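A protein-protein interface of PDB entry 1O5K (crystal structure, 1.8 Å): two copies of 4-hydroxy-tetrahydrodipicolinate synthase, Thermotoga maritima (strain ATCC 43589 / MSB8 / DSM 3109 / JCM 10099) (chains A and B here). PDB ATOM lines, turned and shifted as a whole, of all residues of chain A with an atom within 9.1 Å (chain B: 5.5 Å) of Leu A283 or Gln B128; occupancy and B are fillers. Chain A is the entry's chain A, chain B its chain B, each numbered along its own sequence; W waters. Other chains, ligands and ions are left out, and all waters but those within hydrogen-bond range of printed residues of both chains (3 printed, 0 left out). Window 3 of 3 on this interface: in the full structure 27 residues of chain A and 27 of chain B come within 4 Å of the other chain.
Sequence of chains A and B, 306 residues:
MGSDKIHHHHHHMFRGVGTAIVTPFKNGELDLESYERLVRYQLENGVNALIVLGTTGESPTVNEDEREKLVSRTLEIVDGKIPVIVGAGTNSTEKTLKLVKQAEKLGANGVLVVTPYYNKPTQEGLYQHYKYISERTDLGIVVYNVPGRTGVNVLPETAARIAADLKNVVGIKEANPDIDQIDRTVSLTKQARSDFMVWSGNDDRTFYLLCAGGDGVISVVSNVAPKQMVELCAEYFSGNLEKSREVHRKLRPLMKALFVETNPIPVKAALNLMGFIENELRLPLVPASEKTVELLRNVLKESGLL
The backbone carbonyl oxygen (O) of Leu A283 sits close to the side-chain hydroxyl (OG1) of Thr B93, at 3.3 Å. The backbone nitrogen of Pro A284 sits close to the side-chain hydroxyl of Thr B93 (3.2 Å).
The side-chain hydroxyl of Ser B92 lies close to the backbone NH of Glu B94 (3.4 Å). A ring nitrogen (ND1) of His B129 lies within hydrogen-bond range of the side-chain hydroxyl of Thr B93, at 2.8 Å. NE2 of Gln B128 is in hydrogen-bond range of OE2 of Glu B124, 2.8 Å away.
Among the printed residues, merely in contact across the chains: Pro A284 with Asn B91 (3.2 Å), Pro A284 with Gly B125 (3.3 Å), Pro A60 with Ser B92 (3.5 Å), Pro A60 with Asn B91 (3.5 Å) and Leu A283 with Gln B128 (3.8 Å).
Printed residues of chain B within 4 Å of Pro A60: Asn B91 (3.5 Å) and Ser B92 (3.5 Å). Leu A283 touches just these residues of chain B: Thr B93 and Gln B128. Of the printed residues of chain B, Pro A284 touches Asn B91 (3.2 Å), Thr B93 (3.2 Å) and Gly B125 (3.3 Å). Of the printed residues of chain A, Asn B91 touches Pro A60 and Pro A284. Printed residues of chain A within 4 Å of Gly B125: Pro A284. Of chain A, only Leu A283 (3.8 Å) comes within 4 Å of Gln B128. No residue of chain A comes within 4 Å of Lys B131. The nearest printed residue of chain B that does not touch Leu A283 is Tyr B132 (4.4 Å). The nearest residue of chain A that does not touch Gln B128 is Val A286 (4.6 Å). The nearest printed residue of chain B that does not touch Pro A284 is His B129 (4.2 Å).
Printed residues of chain B that touch a printed residue of chain A: Asn B91, Ser B92, Thr B93, Gly B125 and Gln B128. Of the 14 printed residues of chain A, 3 touch a printed residue of chain B. Hydrophobic or aromatic side chains of chain A that line the printed part of chain B: Pro A60, Leu A283 and Pro A284. Among the printed residues, 7 pairs touch across the chains. Among the printed residues, no Asp or Glu carboxylate lies within 4 Å of a Lys or Arg side-chain nitrogen of the other chain.
No position is printed for both chains. Of the 7 pairs that touch across the chains among the printed residues, none has its exchanged pair printed and touching as well.
Water W2 bridges the backbone carbonyl oxygen of Pro A60 (2.7 Å) and the side-chain amide oxygen of Asn B91 (2.8 Å). Water W3 lies within hydrogen-bond range of the backbone carbonyl oxygen (O) of Leu A283, the backbone NH (N) of Glu B94 and the backbone NH (N) of Thr B93. Water W1 lies within hydrogen-bond range of OE2 of Glu B94 (2.9 Å) and O of Thr A61 (3.0 Å).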
ATOM      1  N   PHE A  25     -25.043   9.132 -11.691  1.00  0.00           N
ATOM      2  CA  PHE A  25     -25.270   7.867 -12.310  1.00  0.00           C
ATOM      3  C   PHE A  25     -26.415   7.172 -11.650  1.00  0.00           C
ATOM      4  O   PHE A  25     -26.671   7.359 -10.447  1.00  0.00           O
ATOM      5  CB  PHE A  25     -24.052   6.931 -12.185  1.00  0.00           C
ATOM      6  CG  PHE A  25     -22.744   7.522 -12.721  1.00  0.00           C
ATOM      7  CD1 PHE A  25     -21.634   7.699 -11.885  1.00  0.00           C
ATOM      8  CD2 PHE A  25     -22.624   7.896 -14.053  1.00  0.00           C
ATOM      9  CE1 PHE A  25     -20.453   8.225 -12.368  1.00  0.00           C
ATOM     10  CE2 PHE A  25     -21.451   8.444 -14.519  1.00  0.00           C
ATOM     11  CZ  PHE A  25     -20.370   8.602 -13.716  1.00  0.00           C
ATOM     12  N   GLY A  28     -25.332   2.603 -12.945  1.00  0.00           N
ATOM     13  CA  GLY A  28     -24.080   2.787 -13.639  1.00  0.00           C
ATOM     14  C   GLY A  28     -24.154   3.594 -14.911  1.00  0.00           C
ATOM     15  O   GLY A  28     -23.118   3.881 -15.486  1.00  0.00           O
ATOM     16  N   GLU A  58     -16.057  13.044 -12.206  1.00  0.00           N
ATOM     17  CA  GLU A  58     -15.567  11.693 -12.586  1.00  0.00           C
ATOM     18  C   GLU A  58     -15.153  11.594 -14.043  1.00  0.00           C
ATOM     19  O   GLU A  58     -15.341  10.559 -14.686  1.00  0.00           O
ATOM     20  CB  GLU A  58     -16.561  10.599 -12.200  1.00  0.00           C
ATOM     21  CG  GLU A  58     -16.568  10.406 -10.703  1.00  0.00           C
ATOM     22  CD  GLU A  58     -17.667   9.522 -10.202  1.00  0.00           C
ATOM     23  OE1 GLU A  58     -18.693  10.100  -9.738  1.00  0.00           O
ATOM     24  OE2 GLU A  58     -17.488   8.273 -10.270  1.00  0.00           O
ATOM     25  N   PRO A  60     -12.427  10.734 -15.406  1.00  0.00           N
ATOM     26  CA  PRO A  60     -11.689   9.544 -15.817  1.00  0.00           C
ATOM     27  C   PRO A  60     -12.564   8.383 -16.274  1.00  0.00           C
ATOM     28  O   PRO A  60     -12.122   7.587 -17.087  1.00  0.00           O
ATOM     29  CB  PRO A  60     -10.902   9.154 -14.538  1.00  0.00           C
ATOM     30  CG  PRO A  60     -10.738  10.400 -13.875  1.00  0.00           C
ATOM     31  CD  PRO A  60     -12.076  11.112 -14.031  1.00  0.00           C
ATOM     32  N   THR A  61     -13.808   8.318 -15.791  1.00  0.00           N
ATOM     33  CA  THR A  61     -14.660   7.181 -16.055  1.00  0.00           C
ATOM     34  C   THR A  61     -15.901   7.455 -16.921  1.00  0.00           C
ATOM     35  O   THR A  61     -16.748   6.563 -17.110  1.00  0.00           O
ATOM     36  CB  THR A  61     -15.108   6.521 -14.747  1.00  0.00           C
ATOM     37  OG1 THR A  61     -15.769   7.474 -13.949  1.00  0.00           O
ATOM     38  CG2 THR A  61     -13.923   6.033 -13.945  1.00  0.00           C
ATOM     39  N   VAL A  62     -15.984   8.657 -17.485  1.00  0.00           N
ATOM     40  CA  VAL A  62     -17.087   9.008 -18.387  1.00  0.00           C
ATOM     41  C   VAL A  62     -16.571   8.923 -19.811  1.00  0.00           C
ATOM     42  O   VAL A  62     -15.595   9.574 -20.155  1.00  0.00           O
ATOM     43  CB  VAL A  62     -17.582  10.400 -18.073  1.00  0.00           C
ATOM     44  CG1 VAL A  62     -18.662  10.820 -19.053  1.00  0.00           C
ATOM     45  CG2 VAL A  62     -18.152  10.428 -16.632  1.00  0.00           C
ATOM     46  N   GLU A 280     -23.989   6.671  -6.376  1.00  0.00           N
ATOM     47  CA  GLU A 280     -23.330   5.692  -7.256  1.00  0.00           C
ATOM     48  C   GLU A 280     -22.116   6.373  -7.840  1.00  0.00           C
ATOM     49  O   GLU A 280     -22.197   7.541  -8.250  1.00  0.00           O
ATOM     50  CB  GLU A 280     -24.224   5.275  -8.416  1.00  0.00           C
ATOM     51  CG  GLU A 280     -25.369   4.360  -8.086  1.00  0.00           C
ATOM     52  CD  GLU A 280     -25.947   3.732  -9.336  1.00  0.00           C
ATOM     53  OE1 GLU A 280     -25.206   3.498 -10.337  1.00  0.00           O
ATOM     54  OE2 GLU A 280     -27.142   3.479  -9.311  1.00  0.00           O
ATOM     55  N   LEU A 281     -21.014   5.624  -7.902  1.00  0.00           N
ATOM     56  CA  LEU A 281     -19.782   6.091  -8.498  1.00  0.00           C
ATOM     57  C   LEU A 281     -19.299   5.003  -9.430  1.00  0.00           C
ATOM     58  O   LEU A 281     -19.787   3.889  -9.399  1.00  0.00           O
ATOM     59  CB  LEU A 281     -18.707   6.347  -7.434  1.00  0.00           C
ATOM     60  CG  LEU A 281     -19.090   7.527  -6.515  1.00  0.00           C
ATOM     61  CD1 LEU A 281     -19.637   7.108  -5.201  1.00  0.00           C
ATOM     62  CD2 LEU A 281     -17.975   8.542  -6.370  1.00  0.00           C
ATOM     63  N   ARG A 282     -18.362   5.338 -10.297  1.00  0.00           N
ATOM     64  CA  ARG A 282     -17.764   4.272 -11.107  1.00  0.00           C
ATOM     65  C   ARG A 282     -16.353   3.863 -10.606  1.00  0.00           C
ATOM     66  O   ARG A 282     -15.525   4.744 -10.203  1.00  0.00           O
ATOM     67  CB  ARG A 282     -17.665   4.755 -12.528  1.00  0.00           C
ATOM     68  CG  ARG A 282     -19.003   4.816 -13.195  1.00  0.00           C
ATOM     69  CD  ARG A 282     -18.926   5.267 -14.621  1.00  0.00           C
ATOM     70  NE  ARG A 282     -20.247   5.281 -15.247  1.00  0.00           N
ATOM     71  CZ  ARG A 282     -20.482   5.754 -16.462  1.00  0.00           C
ATOM     72  NH1 ARG A 282     -19.487   6.233 -17.209  1.00  0.00           N
ATOM     73  NH2 ARG A 282     -21.702   5.712 -16.948  1.00  0.00           N
ATOM     74  N   LEU A 283     -16.068   2.581 -10.706  1.00  0.00           N
ATOM     75  CA  LEU A 283     -14.792   2.033 -10.274  1.00  0.00           C
ATOM     76  C   LEU A 283     -13.687   2.743 -11.062  1.00  0.00           C
ATOM     77  O   LEU A 283     -13.860   3.016 -12.270  1.00  0.00           O
ATOM     78  CB  LEU A 283     -14.760   0.494 -10.493  1.00  0.00           C
ATOM     79  CG  LEU A 283     -15.525  -0.358  -9.490  1.00  0.00           C
ATOM     80  CD1 LEU A 283     -15.318  -1.776  -9.843  1.00  0.00           C
ATOM     81  CD2 LEU A 283     -15.019  -0.077  -8.062  1.00  0.00           C
ATOM     82  N   PRO A 284     -12.557   3.084 -10.421  1.00  0.00           N
ATOM     83  CA  PRO A 284     -12.163   2.642  -9.075  1.00  0.00           C
ATOM     84  C   PRO A 284     -12.734   3.418  -7.859  1.00  0.00           C
ATOM     85  O   PRO A 284     -12.304   3.130  -6.750  1.00  0.00           O
ATOM     86  CB  PRO A 284     -10.644   2.827  -9.111  1.00  0.00           C
ATOM     87  CG  PRO A 284     -10.486   4.060  -9.972  1.00  0.00           C
ATOM     88  CD  PRO A 284     -11.488   3.872 -11.061  1.00  0.00           C
ATOM     89  N   LEU A 285     -13.700   4.317  -8.064  1.00  0.00           N
ATOM     90  CA  LEU A 285     -14.346   4.983  -6.954  1.00  0.00           C
ATOM     91  C   LEU A 285     -15.489   4.114  -6.460  1.00  0.00           C
ATOM     92  O   LEU A 285     -16.053   3.314  -7.217  1.00  0.00           O
ATOM     93  CB  LEU A 285     -14.821   6.383  -7.291  1.00  0.00           C
ATOM     94  CG  LEU A 285     -13.753   7.352  -7.777  1.00  0.00           C
ATOM     95  CD1 LEU A 285     -14.319   8.742  -7.922  1.00  0.00           C
ATOM     96  CD2 LEU A 285     -12.513   7.357  -6.857  1.00  0.00           C
ATOM     97  N   VAL A 286     -15.736   4.211  -5.153  1.00  0.00           N
ATOM     98  CA  VAL A 286     -16.777   3.440  -4.493  1.00  0.00           C
ATOM     99  C   VAL A 286     -17.477   4.363  -3.523  1.00  0.00           C
ATOM    100  O   VAL A 286     -16.940   5.416  -3.194  1.00  0.00           O
ATOM    101  CB  VAL A 286     -16.251   2.229  -3.733  1.00  0.00           C
ATOM    102  CG1 VAL A 286     -15.517   1.210  -4.678  1.00  0.00           C
ATOM    103  CG2 VAL A 286     -15.383   2.668  -2.530  1.00  0.00           C
ATOM    104  N   PRO A 287     -18.707   4.042  -3.139  1.00  0.00           N
ATOM    105  CA  PRO A 287     -19.438   4.862  -2.166  1.00  0.00           C
ATOM    106  C   PRO A 287     -18.764   5.079  -0.805  1.00  0.00           C
ATOM    107  O   PRO A 287     -18.005   4.251  -0.287  1.00  0.00           O
ATOM    108  CB  PRO A 287     -20.758   4.103  -1.988  1.00  0.00           C
ATOM    109  CG  PRO A 287     -20.974   3.439  -3.318  1.00  0.00           C
ATOM    110  CD  PRO A 287     -19.549   2.963  -3.670  1.00  0.00           C
ATOM    111  N   ASN B  91      -6.646   4.957 -15.171  1.00  0.00           N
ATOM    112  CA  ASN B  91      -7.452   5.309 -13.967  1.00  0.00           C
ATOM    113  C   ASN B  91      -8.940   5.024 -14.080  1.00  0.00           C
ATOM    114  O   ASN B  91      -9.705   5.416 -13.193  1.00  0.00           O
ATOM    115  CB  ASN B  91      -7.199   6.754 -13.527  1.00  0.00           C
ATOM    116  CG  ASN B  91      -7.503   7.782 -14.610  1.00  0.00           C
ATOM    117  OD1 ASN B  91      -7.855   7.410 -15.757  1.00  0.00           O
ATOM    118  ND2 ASN B  91      -7.372   9.107 -14.265  1.00  0.00           N
ATOM    119  N   SER B  92      -9.348   4.302 -15.136  1.00  0.00           N
ATOM    120  CA  SER B  92     -10.716   3.782 -15.276  1.00  0.00           C
ATOM    121  C   SER B  92     -10.636   2.267 -15.259  1.00  0.00           C
ATOM    122  O   SER B  92      -9.922   1.664 -16.067  1.00  0.00           O
ATOM    123  CB  SER B  92     -11.328   4.236 -16.600  1.00  0.00           C
ATOM    124  OG  SER B  92     -12.335   3.415 -17.092  1.00  0.00           O
ATOM    125  N   THR B  93     -11.435   1.655 -14.397  1.00  0.00           N
ATOM    126  CA  THR B  93     -11.448   0.204 -14.294  1.00  0.00           C
ATOM    127  C   THR B  93     -11.913  -0.419 -15.605  1.00  0.00           C
ATOM    128  O   THR B  93     -11.294  -1.372 -16.082  1.00  0.00           O
ATOM    129  CB  THR B  93     -12.324  -0.235 -13.141  1.00  0.00           C
ATOM    130  OG1 THR B  93     -11.857   0.390 -11.940  1.00  0.00           O
ATOM    131  CG2 THR B  93     -12.231  -1.738 -12.885  1.00  0.00           C
ATOM    132  N   GLU B  94     -12.956   0.143 -16.207  1.00  0.00           N
ATOM    133  CA  GLU B  94     -13.442  -0.289 -17.493  1.00  0.00           C
ATOM    134  C   GLU B  94     -12.385  -0.265 -18.574  1.00  0.00           C
ATOM    135  O   GLU B  94     -12.210  -1.260 -19.305  1.00  0.00           O
ATOM    136  CB  GLU B  94     -14.661   0.536 -17.886  1.00  0.00           C
ATOM    137  CG  GLU B  94     -15.301   0.117 -19.179  1.00  0.00           C
ATOM    138  CD  GLU B  94     -16.513   0.988 -19.526  1.00  0.00           C
ATOM    139  OE1 GLU B  94     -17.404   0.465 -20.223  1.00  0.00           O
ATOM    140  OE2 GLU B  94     -16.572   2.197 -19.104  1.00  0.00           O
ATOM    141  N   GLN B 123      -8.664   2.609  -0.536  1.00  0.00           N
ATOM    142  CA  GLN B 123      -8.034   1.303  -0.520  1.00  0.00           C
ATOM    143  C   GLN B 123      -8.987   0.209  -1.010  1.00  0.00           C
ATOM    144  O   GLN B 123      -8.574  -0.722  -1.683  1.00  0.00           O
ATOM    145  CB  GLN B 123      -7.478   0.987   0.879  1.00  0.00           C
ATOM    146  CG  GLN B 123      -6.347   1.940   1.315  1.00  0.00           C
ATOM    147  CD  GLN B 123      -5.100   1.889   0.484  1.00  0.00           C
ATOM    148  OE1 GLN B 123      -4.431   0.830   0.396  1.00  0.00           O
ATOM    149  NE2 GLN B 123      -4.736   3.041  -0.139  1.00  0.00           N
ATOM    150  N   GLU B 124     -10.243   0.286  -0.596  1.00  0.00           N
ATOM    151  CA  GLU B 124     -11.250  -0.673  -1.045  1.00  0.00           C
ATOM    152  C   GLU B 124     -11.427  -0.532  -2.558  1.00  0.00           C
ATOM    153  O   GLU B 124     -11.572  -1.526  -3.244  1.00  0.00           O
ATOM    154  CB  GLU B 124     -12.563  -0.440  -0.302  1.00  0.00           C
ATOM    155  CG  GLU B 124     -13.735  -1.334  -0.717  1.00  0.00           C
ATOM    156  CD  GLU B 124     -13.492  -2.825  -0.483  1.00  0.00           C
ATOM    157  OE1 GLU B 124     -12.610  -3.144   0.323  1.00  0.00           O
ATOM    158  OE2 GLU B 124     -14.200  -3.681  -1.082  1.00  0.00           O
ATOM    159  N   GLY B 125     -11.416   0.692  -3.076  1.00  0.00           N
ATOM    160  CA  GLY B 125     -11.495   0.894  -4.517  1.00  0.00           C
ATOM    161  C   GLY B 125     -10.367   0.260  -5.276  1.00  0.00           C
ATOM    162  O   GLY B 125     -10.555  -0.302  -6.379  1.00  0.00           O
ATOM    163  N   LEU B 126      -9.167   0.381  -4.736  1.00  0.00           N
ATOM    164  CA  LEU B 126      -8.013  -0.293  -5.328  1.00  0.00           C
ATOM    165  C   LEU B 126      -8.232  -1.803  -5.365  1.00  0.00           C
ATOM    166  O   LEU B 126      -8.035  -2.438  -6.408  1.00  0.00           O
ATOM    167  CB  LEU B 126      -6.731   0.028  -4.573  1.00  0.00           C
ATOM    168  CG  LEU B 126      -6.167   1.469  -4.741  1.00  0.00           C
ATOM    169  CD1 LEU B 126      -5.039   1.707  -3.817  1.00  0.00           C
ATOM    170  CD2 LEU B 126      -5.760   1.722  -6.235  1.00  0.00           C
ATOM    171  N   TYR B 127      -8.653  -2.368  -4.240  1.00  0.00           N
ATOM    172  CA  TYR B 127      -8.943  -3.784  -4.188  1.00  0.00           C
ATOM    173  C   TYR B 127     -10.009  -4.187  -5.220  1.00  0.00           C
ATOM    174  O   TYR B 127      -9.818  -5.138  -5.964  1.00  0.00           O
ATOM    175  CB  TYR B 127      -9.383  -4.174  -2.793  1.00  0.00           C
ATOM    176  CG  TYR B 127      -9.843  -5.611  -2.684  1.00  0.00           C
ATOM    177  CD1 TYR B 127      -8.942  -6.631  -2.451  1.00  0.00           C
ATOM    178  CD2 TYR B 127     -11.198  -5.930  -2.773  1.00  0.00           C
ATOM    179  CE1 TYR B 127      -9.368  -7.945  -2.316  1.00  0.00           C
ATOM    180  CE2 TYR B 127     -11.639  -7.258  -2.652  1.00  0.00           C
ATOM    181  CZ  TYR B 127     -10.702  -8.247  -2.419  1.00  0.00           C
ATOM    182  OH  TYR B 127     -11.099  -9.558  -2.304  1.00  0.00           O
ATOM    183  N   GLN B 128     -11.124  -3.466  -5.248  1.00  0.00           N
ATOM    184  CA  GLN B 128     -12.186  -3.728  -6.238  1.00  0.00           C
ATOM    185  C   GLN B 128     -11.741  -3.587  -7.678  1.00  0.00           C
ATOM    186  O   GLN B 128     -12.213  -4.333  -8.524  1.00  0.00           O
ATOM    187  CB  GLN B 128     -13.405  -2.874  -5.983  1.00  0.00           C
ATOM    188  CG  GLN B 128     -14.098  -3.210  -4.668  1.00  0.00           C
ATOM    189  CD  GLN B 128     -14.660  -4.634  -4.578  1.00  0.00           C
ATOM    190  OE1 GLN B 128     -15.003  -5.245  -5.592  1.00  0.00           O
ATOM    191  NE2 GLN B 128     -14.745  -5.159  -3.360  1.00  0.00           N
ATOM    192  N   HIS B 129     -10.849  -2.627  -7.943  1.00  0.00           N
ATOM    193  CA  HIS B 129     -10.260  -2.390  -9.294  1.00  0.00           C
ATOM    194  C   HIS B 129      -9.531  -3.660  -9.756  1.00  0.00           C
ATOM    195  O   HIS B 129      -9.760  -4.179 -10.852  1.00  0.00           O
ATOM    196  CB  HIS B 129      -9.297  -1.198  -9.187  1.00  0.00           C
ATOM    197  CG  HIS B 129      -8.559  -0.859 -10.465  1.00  0.00           C
ATOM    198  ND1 HIS B 129      -9.178  -0.271 -11.544  1.00  0.00           N
ATOM    199  CD2 HIS B 129      -7.260  -1.008 -10.809  1.00  0.00           C
ATOM    200  CE1 HIS B 129      -8.278  -0.054 -12.501  1.00  0.00           C
ATOM    201  NE2 HIS B 129      -7.102  -0.497 -12.075  1.00  0.00           N
ATOM    202  N   TYR B 130      -8.637  -4.150  -8.907  1.00  0.00           N
ATOM    203  CA  TYR B 130      -7.819  -5.309  -9.280  1.00  0.00           C
ATOM    204  C   TYR B 130      -8.684  -6.538  -9.281  1.00  0.00           C
ATOM    205  O   TYR B 130      -8.461  -7.419 -10.074  1.00  0.00           O
ATOM    206  CB  TYR B 130      -6.605  -5.479  -8.363  1.00  0.00           C
ATOM    207  CG  TYR B 130      -5.571  -4.407  -8.620  1.00  0.00           C
ATOM    208  CD1 TYR B 130      -4.769  -4.444  -9.775  1.00  0.00           C
ATOM    209  CD2 TYR B 130      -5.424  -3.335  -7.785  1.00  0.00           C
ATOM    210  CE1 TYR B 130      -3.836  -3.440 -10.057  1.00  0.00           C
ATOM    211  CE2 TYR B 130      -4.463  -2.303  -8.057  1.00  0.00           C
ATOM    212  CZ  TYR B 130      -3.664  -2.379  -9.214  1.00  0.00           C
ATOM    213  OH  TYR B 130      -2.726  -1.342  -9.459  1.00  0.00           O
ATOM    214  N   LYS B 131      -9.697  -6.595  -8.416  1.00  0.00           N
ATOM    215  CA  LYS B 131     -10.578  -7.763  -8.405  1.00  0.00           C
ATOM    216  C   LYS B 131     -11.408  -7.859  -9.701  1.00  0.00           C
ATOM    217  O   LYS B 131     -11.617  -8.937 -10.284  1.00  0.00           O
ATOM    218  CB  LYS B 131     -11.503  -7.755  -7.157  1.00  0.00           C
ATOM    219  CG  LYS B 131     -12.570  -8.866  -7.157  1.00  0.00           C
ATOM    220  CD  LYS B 131     -13.261  -8.891  -5.811  1.00  0.00           C
ATOM    221  CE  LYS B 131     -14.238 -10.067  -5.644  1.00  0.00           C
ATOM    222  NZ  LYS B 131     -15.511  -9.835  -6.334  1.00  0.00           N
ATOM    223  N   TYR B 132     -11.913  -6.712 -10.143  1.00  0.00           N
ATOM    224  CA  TYR B 132     -12.732  -6.622 -11.352  1.00  0.00           C
ATOM    225  C   TYR B 132     -11.940  -7.129 -12.571  1.00  0.00           C
ATOM    226  O   TYR B 132     -12.467  -7.869 -13.357  1.00  0.00           O
ATOM    227  CB  TYR B 132     -13.142  -5.185 -11.618  1.00  0.00           C
ATOM    228  CG  TYR B 132     -14.095  -5.089 -12.792  1.00  0.00           C
ATOM    229  CD1 TYR B 132     -15.449  -5.355 -12.643  1.00  0.00           C
ATOM    230  CD2 TYR B 132     -13.623  -4.793 -14.059  1.00  0.00           C
ATOM    231  CE1 TYR B 132     -16.328  -5.288 -13.749  1.00  0.00           C
ATOM    232  CE2 TYR B 132     -14.489  -4.745 -15.160  1.00  0.00           C
ATOM    233  CZ  TYR B 132     -15.822  -4.990 -14.998  1.00  0.00           C
ATOM    234  OH  TYR B 132     -16.645  -4.916 -16.109  1.00  0.00           O
ATOM    235  N   ILE B 133     -10.683  -6.719 -12.685  1.00  0.00           N
ATOM    236  CA  ILE B 133      -9.789  -7.090 -13.780  1.00  0.00           C
ATOM    237  C   ILE B 133      -9.376  -8.569 -13.634  1.00  0.00           C
ATOM    238  O   ILE B 133      -9.420  -9.321 -14.622  1.00  0.00           O
ATOM    239  CB  ILE B 133      -8.536  -6.187 -13.792  1.00  0.00           C
ATOM    240  CG1 ILE B 133      -8.941  -4.719 -14.007  1.00  0.00           C
ATOM    241  CG2 ILE B 133      -7.550  -6.589 -14.893  1.00  0.00           C
ATOM    242  CD1 ILE B 133      -7.905  -3.750 -13.475  1.00  0.00           C
HETATM  243  O   HOH W   1     -15.892   3.762 -16.704  1.00  0.00           O
HETATM  244  O   HOH W   2      -9.568   7.512 -17.918  1.00  0.00           O
HETATM  245  O   HOH W   3     -14.799   2.148 -14.642  1.00  0.00           O
